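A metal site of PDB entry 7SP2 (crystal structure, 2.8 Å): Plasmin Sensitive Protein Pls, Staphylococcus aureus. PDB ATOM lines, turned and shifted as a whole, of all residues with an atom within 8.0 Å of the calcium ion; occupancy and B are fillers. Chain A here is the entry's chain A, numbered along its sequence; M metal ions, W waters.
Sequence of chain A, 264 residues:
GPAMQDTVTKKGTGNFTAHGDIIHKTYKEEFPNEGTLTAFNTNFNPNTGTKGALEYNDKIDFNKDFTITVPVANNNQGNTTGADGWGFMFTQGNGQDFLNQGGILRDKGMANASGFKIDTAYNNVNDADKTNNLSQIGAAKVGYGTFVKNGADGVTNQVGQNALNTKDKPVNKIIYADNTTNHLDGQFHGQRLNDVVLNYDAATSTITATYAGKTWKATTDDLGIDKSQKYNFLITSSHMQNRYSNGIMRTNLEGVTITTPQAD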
ATOM      1  N   ASN A  79      10.131  16.354   0.431  1.00  0.00           N
ATOM      2  CA  ASN A  79      11.067  15.293  -0.002  1.00  0.00           C
ATOM      3  C   ASN A  79      12.407  15.319   0.776  1.00  0.00           C
ATOM      4  O   ASN A  79      13.180  14.365   0.625  1.00  0.00           O
ATOM      5  CB  ASN A  79      11.184  15.359  -1.518  1.00  0.00           C
ATOM      6  CG  ASN A  79      11.864  16.606  -2.043  1.00  0.00           C
ATOM      7  OD1 ASN A  79      12.594  17.290  -1.340  1.00  0.00           O
ATOM      8  ND2 ASN A  79      11.624  16.884  -3.308  1.00  0.00           N
ATOM      9  N   ALA A  83       9.551   9.852   3.764  1.00  0.00           N
ATOM     10  CA  ALA A  83      10.002   8.495   3.419  1.00  0.00           C
ATOM     11  C   ALA A  83      10.724   8.535   2.077  1.00  0.00           C
ATOM     12  O   ALA A  83      10.521   9.465   1.263  1.00  0.00           O
ATOM     13  CB  ALA A  83       8.817   7.549   3.366  1.00  0.00           C
ATOM     14  N   ASP A  84      11.482   7.470   1.841  1.00  0.00           N
ATOM     15  CA  ASP A  84      12.304   7.298   0.614  1.00  0.00           C
ATOM     16  C   ASP A  84      11.376   7.076  -0.569  1.00  0.00           C
ATOM     17  O   ASP A  84      11.753   7.478  -1.688  1.00  0.00           O
ATOM     18  CB  ASP A  84      13.264   6.130   0.780  1.00  0.00           C
ATOM     19  CG  ASP A  84      14.331   6.356   1.821  1.00  0.00           C
ATOM     20  OD1 ASP A  84      14.721   7.537   2.030  1.00  0.00           O
ATOM     21  OD2 ASP A  84      14.788   5.347   2.395  1.00  0.00           O
ATOM     22  N   GLY A  85      10.245   6.421  -0.330  1.00  0.00           N
ATOM     23  CA  GLY A  85       9.239   6.143  -1.358  1.00  0.00           C
ATOM     24  C   GLY A  85       8.795   4.696  -1.313  1.00  0.00           C
ATOM     25  O   GLY A  85       8.725   4.095  -0.202  1.00  0.00           O
ATOM     26  N   ILE A 104      15.814  -0.746  -3.263  1.00  0.00           N
ATOM     27  CA  ILE A 104      15.981  -0.100  -4.596  1.00  0.00           C
ATOM     28  C   ILE A 104      15.652   1.391  -4.497  1.00  0.00           C
ATOM     29  O   ILE A 104      15.505   2.028  -5.548  1.00  0.00           O
ATOM     30  CB  ILE A 104      15.162  -0.824  -5.672  1.00  0.00           C
ATOM     31  CG1 ILE A 104      13.670  -0.878  -5.358  1.00  0.00           C
ATOM     32  CG2 ILE A 104      15.691  -2.222  -5.912  1.00  0.00           C
ATOM     33  CD1 ILE A 104      12.823  -1.212  -6.575  1.00  0.00           C
ATOM     34  N   LEU A 105      15.588   1.961  -3.299  1.00  0.00           N
ATOM     35  CA  LEU A 105      15.160   3.376  -3.148  1.00  0.00           C
ATOM     36  C   LEU A 105      16.333   4.324  -2.885  1.00  0.00           C
ATOM     37  O   LEU A 105      16.090   5.542  -2.755  1.00  0.00           O
ATOM     38  CB  LEU A 105      14.147   3.403  -2.012  1.00  0.00           C
ATOM     39  CG  LEU A 105      12.732   3.032  -2.424  1.00  0.00           C
ATOM     40  CD1 LEU A 105      11.865   2.776  -1.210  1.00  0.00           C
ATOM     41  CD2 LEU A 105      12.127   4.144  -3.258  1.00  0.00           C
ATOM     42  N   ARG A 106      17.551   3.798  -2.784  1.00  0.00           N
ATOM     43  CA  ARG A 106      18.740   4.597  -2.417  1.00  0.00           C
ATOM     44  C   ARG A 106      19.789   4.329  -3.449  1.00  0.00           C
ATOM     45  O   ARG A 106      19.404   4.082  -4.573  1.00  0.00           O
ATOM     46  CB  ARG A 106      19.162   4.254  -1.001  1.00  0.00           C
ATOM     47  CG  ARG A 106      18.254   4.928   0.016  1.00  0.00           C
ATOM     48  CD  ARG A 106      18.007   3.801   0.934  1.00  0.00           C
ATOM     49  NE  ARG A 106      17.391   4.108   2.199  1.00  0.00           N
ATOM     50  CZ  ARG A 106      18.003   4.698   3.193  1.00  0.00           C
ATOM     51  NH1 ARG A 106      19.255   5.130   3.045  1.00  0.00           N
ATOM     52  NH2 ARG A 106      17.362   4.885   4.334  1.00  0.00           N
ATOM     53  N   ASP A 107      21.073   4.413  -3.117  1.00  0.00           N
ATOM     54  CA  ASP A 107      22.128   4.205  -4.141  1.00  0.00           C
ATOM     55  C   ASP A 107      22.582   2.741  -4.137  1.00  0.00           C
ATOM     56  O   ASP A 107      23.186   2.366  -5.123  1.00  0.00           O
ATOM     57  CB  ASP A 107      23.299   5.182  -3.990  1.00  0.00           C
ATOM     58  CG  ASP A 107      24.074   4.979  -2.705  1.00  0.00           C
ATOM     59  OD1 ASP A 107      23.539   4.290  -1.799  1.00  0.00           O
ATOM     60  OD2 ASP A 107      25.202   5.506  -2.626  1.00  0.00           O
ATOM     61  N   LYS A 117      10.370   2.106  -8.781  1.00  0.00           N
ATOM     62  CA  LYS A 117      10.355   2.945  -7.573  1.00  0.00           C
ATOM     63  C   LYS A 117       9.520   4.178  -7.829  1.00  0.00           C
ATOM     64  O   LYS A 117       9.594   4.758  -8.931  1.00  0.00           O
ATOM     65  CB  LYS A 117      11.747   3.318  -7.058  1.00  0.00           C
ATOM     66  CG  LYS A 117      12.540   4.330  -7.862  1.00  0.00           C
ATOM     67  CD  LYS A 117      13.814   4.757  -7.147  1.00  0.00           C
ATOM     68  CE  LYS A 117      14.623   5.789  -7.903  1.00  0.00           C
ATOM     69  NZ  LYS A 117      15.679   6.434  -7.079  1.00  0.00           N
ATOM     70  N   ILE A 118       8.705   4.529  -6.831  1.00  0.00           N
ATOM     71  CA  ILE A 118       8.197   5.896  -6.614  1.00  0.00           C
ATOM     72  C   ILE A 118       9.141   6.516  -5.594  1.00  0.00           C
ATOM     73  O   ILE A 118       9.118   6.085  -4.450  1.00  0.00           O
ATOM     74  CB  ILE A 118       6.746   5.842  -6.140  1.00  0.00           C
ATOM     75  CG1 ILE A 118       5.871   5.140  -7.152  1.00  0.00           C
ATOM     76  CG2 ILE A 118       6.227   7.210  -5.838  1.00  0.00           C
ATOM     77  CD1 ILE A 118       4.490   4.814  -6.616  1.00  0.00           C
ATOM     78  N   ASP A 119      10.022   7.378  -6.038  1.00  0.00           N
ATOM     79  CA  ASP A 119      11.054   7.984  -5.191  1.00  0.00           C
ATOM     80  C   ASP A 119      10.463   9.275  -4.658  1.00  0.00           C
ATOM     81  O   ASP A 119      10.121  10.150  -5.454  1.00  0.00           O
ATOM     82  CB  ASP A 119      12.335   8.211  -5.992  1.00  0.00           C
ATOM     83  CG  ASP A 119      13.510   8.603  -5.099  1.00  0.00           C
ATOM     84  OD1 ASP A 119      13.320   9.455  -4.217  1.00  0.00           O
ATOM     85  OD2 ASP A 119      14.604   8.059  -5.249  1.00  0.00           O
ATOM     86  N   THR A 120      10.345   9.378  -3.344  1.00  0.00           N
ATOM     87  CA  THR A 120       9.654  10.513  -2.713  1.00  0.00           C
ATOM     88  C   THR A 120      10.625  11.281  -1.843  1.00  0.00           C
ATOM     89  O   THR A 120      10.168  12.061  -0.988  1.00  0.00           O
ATOM     90  CB  THR A 120       8.456  10.024  -1.891  1.00  0.00           C
ATOM     91  OG1 THR A 120       8.910   9.097  -0.905  1.00  0.00           O
ATOM     92  CG2 THR A 120       7.421   9.388  -2.782  1.00  0.00           C
ATOM     93  N   ALA A 121      11.924  11.052  -2.033  1.00  0.00           N
ATOM     94  CA  ALA A 121      12.949  11.698  -1.182  1.00  0.00           C
ATOM     95  C   ALA A 121      14.115  12.188  -2.021  1.00  0.00           C
ATOM     96  O   ALA A 121      14.591  11.468  -2.908  1.00  0.00           O
ATOM     97  CB  ALA A 121      13.440  10.751  -0.126  1.00  0.00           C
ATOM     98  N   TYR A 122      14.594  13.367  -1.689  1.00  0.00           N
ATOM     99  CA  TYR A 122      15.879  13.886  -2.183  1.00  0.00           C
ATOM    100  C   TYR A 122      16.913  13.453  -1.164  1.00  0.00           C
ATOM    101  O   TYR A 122      16.932  14.040  -0.068  1.00  0.00           O
ATOM    102  CB  TYR A 122      15.812  15.398  -2.338  1.00  0.00           C
ATOM    103  CG  TYR A 122      17.015  16.008  -2.968  1.00  0.00           C
ATOM    104  CD1 TYR A 122      17.171  16.004  -4.347  1.00  0.00           C
ATOM    105  CD2 TYR A 122      17.987  16.626  -2.214  1.00  0.00           C
ATOM    106  CE1 TYR A 122      18.253  16.608  -4.969  1.00  0.00           C
ATOM    107  CE2 TYR A 122      19.079  17.240  -2.819  1.00  0.00           C
ATOM    108  CZ  TYR A 122      19.221  17.236  -4.201  1.00  0.00           C
ATOM    109  OH  TYR A 122      20.280  17.821  -4.823  1.00  0.00           O
ATOM    110  N   ASN A 123      17.614  12.380  -1.505  1.00  0.00           N
ATOM    111  CA  ASN A 123      18.629  11.746  -0.637  1.00  0.00           C
ATOM    112  C   ASN A 123      19.858  11.224  -1.382  1.00  0.00           C
ATOM    113  O   ASN A 123      20.762  10.842  -0.691  1.00  0.00           O
ATOM    114  CB  ASN A 123      18.151  10.525   0.154  1.00  0.00           C
ATOM    115  CG  ASN A 123      17.073   9.592  -0.398  1.00  0.00           C
ATOM    116  OD1 ASN A 123      16.559   9.689  -1.506  1.00  0.00           O
ATOM    117  ND2 ASN A 123      16.703   8.658   0.451  1.00  0.00           N
ATOM    118  N   ASN A 124      19.926  11.093  -2.703  1.00  0.00           N
ATOM    119  CA  ASN A 124      21.025  10.286  -3.313  1.00  0.00           C
ATOM    120  C   ASN A 124      21.598  10.931  -4.569  1.00  0.00           C
ATOM    121  O   ASN A 124      20.966  11.796  -5.142  1.00  0.00           O
ATOM    122  CB  ASN A 124      20.554   8.867  -3.617  1.00  0.00           C
ATOM    123  CG  ASN A 124      20.543   7.996  -2.381  1.00  0.00           C
ATOM    124  OD1 ASN A 124      19.518   7.720  -1.798  1.00  0.00           O
ATOM    125  ND2 ASN A 124      21.716   7.594  -1.971  1.00  0.00           N
ATOM    126  N   VAL A 125      22.743  10.474  -5.053  1.00  0.00           N
ATOM    127  CA  VAL A 125      23.254  11.040  -6.333  1.00  0.00           C
ATOM    128  C   VAL A 125      22.212  10.842  -7.455  1.00  0.00           C
ATOM    129  O   VAL A 125      22.040  11.833  -8.172  1.00  0.00           O
ATOM    130  CB  VAL A 125      24.655  10.526  -6.717  1.00  0.00           C
ATOM    131  CG1 VAL A 125      25.676  11.351  -6.010  1.00  0.00           C
ATOM    132  CG2 VAL A 125      24.840   9.042  -6.409  1.00  0.00           C
ATOM    133  N   ASN A 126      21.528   9.681  -7.598  1.00  0.00           N
ATOM    134  CA  ASN A 126      20.569   9.421  -8.730  1.00  0.00           C
ATOM    135  C   ASN A 126      19.418  10.455  -8.738  1.00  0.00           C
ATOM    136  O   ASN A 126      18.939  10.791  -9.817  1.00  0.00           O
ATOM    137  CB  ASN A 126      20.059   7.975  -8.787  1.00  0.00           C
ATOM    138  CG  ASN A 126      19.544   7.379  -7.470  1.00  0.00           C
ATOM    139  OD1 ASN A 126      18.459   7.704  -6.974  1.00  0.00           O
ATOM    140  ND2 ASN A 126      20.303   6.450  -6.910  1.00  0.00           N
ATOM    141  N   ASP A 127      18.965  10.916  -7.582  1.00  0.00           N
ATOM    142  CA  ASP A 127      18.021  12.046  -7.314  1.00  0.00           C
ATOM    143  C   ASP A 127      18.523  13.378  -7.879  1.00  0.00           C
ATOM    144  O   ASP A 127      17.764  14.341  -7.849  1.00  0.00           O
ATOM    145  CB  ASP A 127      17.894  12.241  -5.790  1.00  0.00           C
ATOM    146  CG  ASP A 127      17.200  11.136  -5.006  1.00  0.00           C
ATOM    147  OD1 ASP A 127      16.370  10.456  -5.599  1.00  0.00           O
ATOM    148  OD2 ASP A 127      17.437  10.958  -3.773  1.00  0.00           O
ATOM    149  N   ALA A 128      19.786  13.479  -8.240  1.00  0.00           N
ATOM    150  CA  ALA A 128      20.455  14.768  -8.554  1.00  0.00           C
ATOM    151  C   ALA A 128      20.120  15.178  -9.983  1.00  0.00           C
ATOM    152  O   ALA A 128      20.416  16.337 -10.348  1.00  0.00           O
ATOM    153  CB  ALA A 128      21.954  14.675  -8.339  1.00  0.00           C
ATOM    154  N   LEU A 134      14.268  15.202 -10.957  1.00  0.00           N
ATOM    155  CA  LEU A 134      13.879  16.002  -9.787  1.00  0.00           C
ATOM    156  C   LEU A 134      14.581  17.352  -9.812  1.00  0.00           C
ATOM    157  O   LEU A 134      15.790  17.376  -9.951  1.00  0.00           O
ATOM    158  CB  LEU A 134      14.258  15.159  -8.567  1.00  0.00           C
ATOM    159  CG  LEU A 134      13.849  15.711  -7.207  1.00  0.00           C
ATOM    160  CD1 LEU A 134      12.360  16.035  -7.164  1.00  0.00           C
ATOM    161  CD2 LEU A 134      14.240  14.677  -6.143  1.00  0.00           C
ATOM    162  N   GLY A 143       8.528  14.063  -6.164  1.00  0.00           N
ATOM    163  CA  GLY A 143       9.505  13.003  -6.393  1.00  0.00           C
ATOM    164  C   GLY A 143       9.451  12.594  -7.820  1.00  0.00           C
ATOM    165  O   GLY A 143       9.199  13.446  -8.699  1.00  0.00           O
ATOM    166  N   TYR A 144       9.675  11.325  -8.065  1.00  0.00           N
ATOM    167  CA  TYR A 144       9.730  10.834  -9.451  1.00  0.00           C
ATOM    168  C   TYR A 144       9.548   9.338  -9.445  1.00  0.00           C
ATOM    169  O   TYR A 144       9.827   8.687  -8.443  1.00  0.00           O
ATOM    170  CB  TYR A 144      11.025  11.241 -10.132  1.00  0.00           C
ATOM    171  CG  TYR A 144      12.286  10.728  -9.509  1.00  0.00           C
ATOM    172  CD1 TYR A 144      12.857  11.370  -8.425  1.00  0.00           C
ATOM    173  CD2 TYR A 144      12.936   9.615 -10.028  1.00  0.00           C
ATOM    174  CE1 TYR A 144      14.036  10.899  -7.872  1.00  0.00           C
ATOM    175  CE2 TYR A 144      14.146   9.163  -9.524  1.00  0.00           C
ATOM    176  CZ  TYR A 144      14.699   9.805  -8.431  1.00  0.00           C
ATOM    177  OH  TYR A 144      15.862   9.284  -7.948  1.00  0.00           O
ATOM    178  N   MET A 240      14.633   7.438   6.051  1.00  0.00           N
ATOM    179  CA  MET A 240      16.049   7.599   6.415  1.00  0.00           C
ATOM    180  C   MET A 240      16.200   7.825   7.925  1.00  0.00           C
ATOM    181  O   MET A 240      15.235   8.289   8.596  1.00  0.00           O
ATOM    182  CB  MET A 240      16.664   8.746   5.628  1.00  0.00           C
ATOM    183  CG  MET A 240      17.547   8.262   4.513  1.00  0.00           C
ATOM    184  SD  MET A 240      17.566   9.543   3.288  1.00  0.00           S
ATOM    185  CE  MET A 240      19.247  10.166   3.479  1.00  0.00           C
ATOM    186  N   ARG A 243      15.967  11.708   9.935  1.00  0.00           N
ATOM    187  CA  ARG A 243      14.722  12.422   9.521  1.00  0.00           C
ATOM    188  C   ARG A 243      13.785  12.358  10.717  1.00  0.00           C
ATOM    189  O   ARG A 243      13.477  11.260  11.226  1.00  0.00           O
ATOM    190  CB  ARG A 243      14.193  11.918   8.189  1.00  0.00           C
ATOM    191  CG  ARG A 243      15.146  12.172   7.031  1.00  0.00           C
ATOM    192  CD  ARG A 243      14.575  11.789   5.677  1.00  0.00           C
ATOM    193  NE  ARG A 243      15.452  12.266   4.596  1.00  0.00           N
ATOM    194  CZ  ARG A 243      15.059  12.639   3.357  1.00  0.00           C
ATOM    195  NH1 ARG A 243      13.779  12.564   2.989  1.00  0.00           N
ATOM    196  NH2 ARG A 243      15.960  13.087   2.491  1.00  0.00           N
HETATM  197 CA    CA M   1      15.576   9.443  -3.614  1.00  0.00          CA
HETATM  198  O   HOH W   1      14.659   7.667  -2.421  1.00  0.00           O
HETATM  199  O   HOH W   2      17.329   7.953  -3.367  1.00  0.00           O
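Within 4 Å of the calcium ion: Asp 119, Ala 121, Asn 123 and Asp 127. The nearest printed residue that does not touch the calcium ion is Leu 105 (4.03 Å).
The backbone NH of Asp 119 sits at hydrogen-bond distance from the backbone carbonyl oxygen of Tyr 144, at 2.7 Å. The side-chain carboxylate of Asp 119 sits close to the side-chain amino group of Lys 117, at 2.7 Å. The side-chain amide nitrogen (ND2) of Asn 123 sits at hydrogen-bond distance from the side-chain carboxylate (OD1) of Asp 84. The side-chain sulfur (SD) of Met 240 is in hydrogen-bond range of the side-chain amide nitrogen (ND2) of Asn 123 (3.1 Å). The side-chain carboxylate of Asp 127 lies close to the side-chain hydroxyl of Tyr 144. The side-chain carboxylate (OD2) of Asp 127 sits close to the backbone NH (N) of Asn 124 (2.7 Å).
The calcium ion is bound by water W2 (2.3 Å), water W1 (2.3 Å), OD1 of Asp 119 (2.3 Å), OD1 of Asn 123 (2.3 Å), OD2 of Asp 119 (2.4 Å), O of Ala 121 (2.4 Å), OD1 of Asp 127 (2.4 Å) and OD2 of Asp 127 (2.4 Å).
Water W2 lies within hydrogen-bond range of the side-chain amide oxygen (OD1) of Asn 124 (2.7 Å) and the backbone carbonyl oxygen (O) of Leu 105 (2.8 Å). Water W1 lies within hydrogen-bond range of O of Leu 105 (2.6 Å) and O of Asp 84 (3.0 Å).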
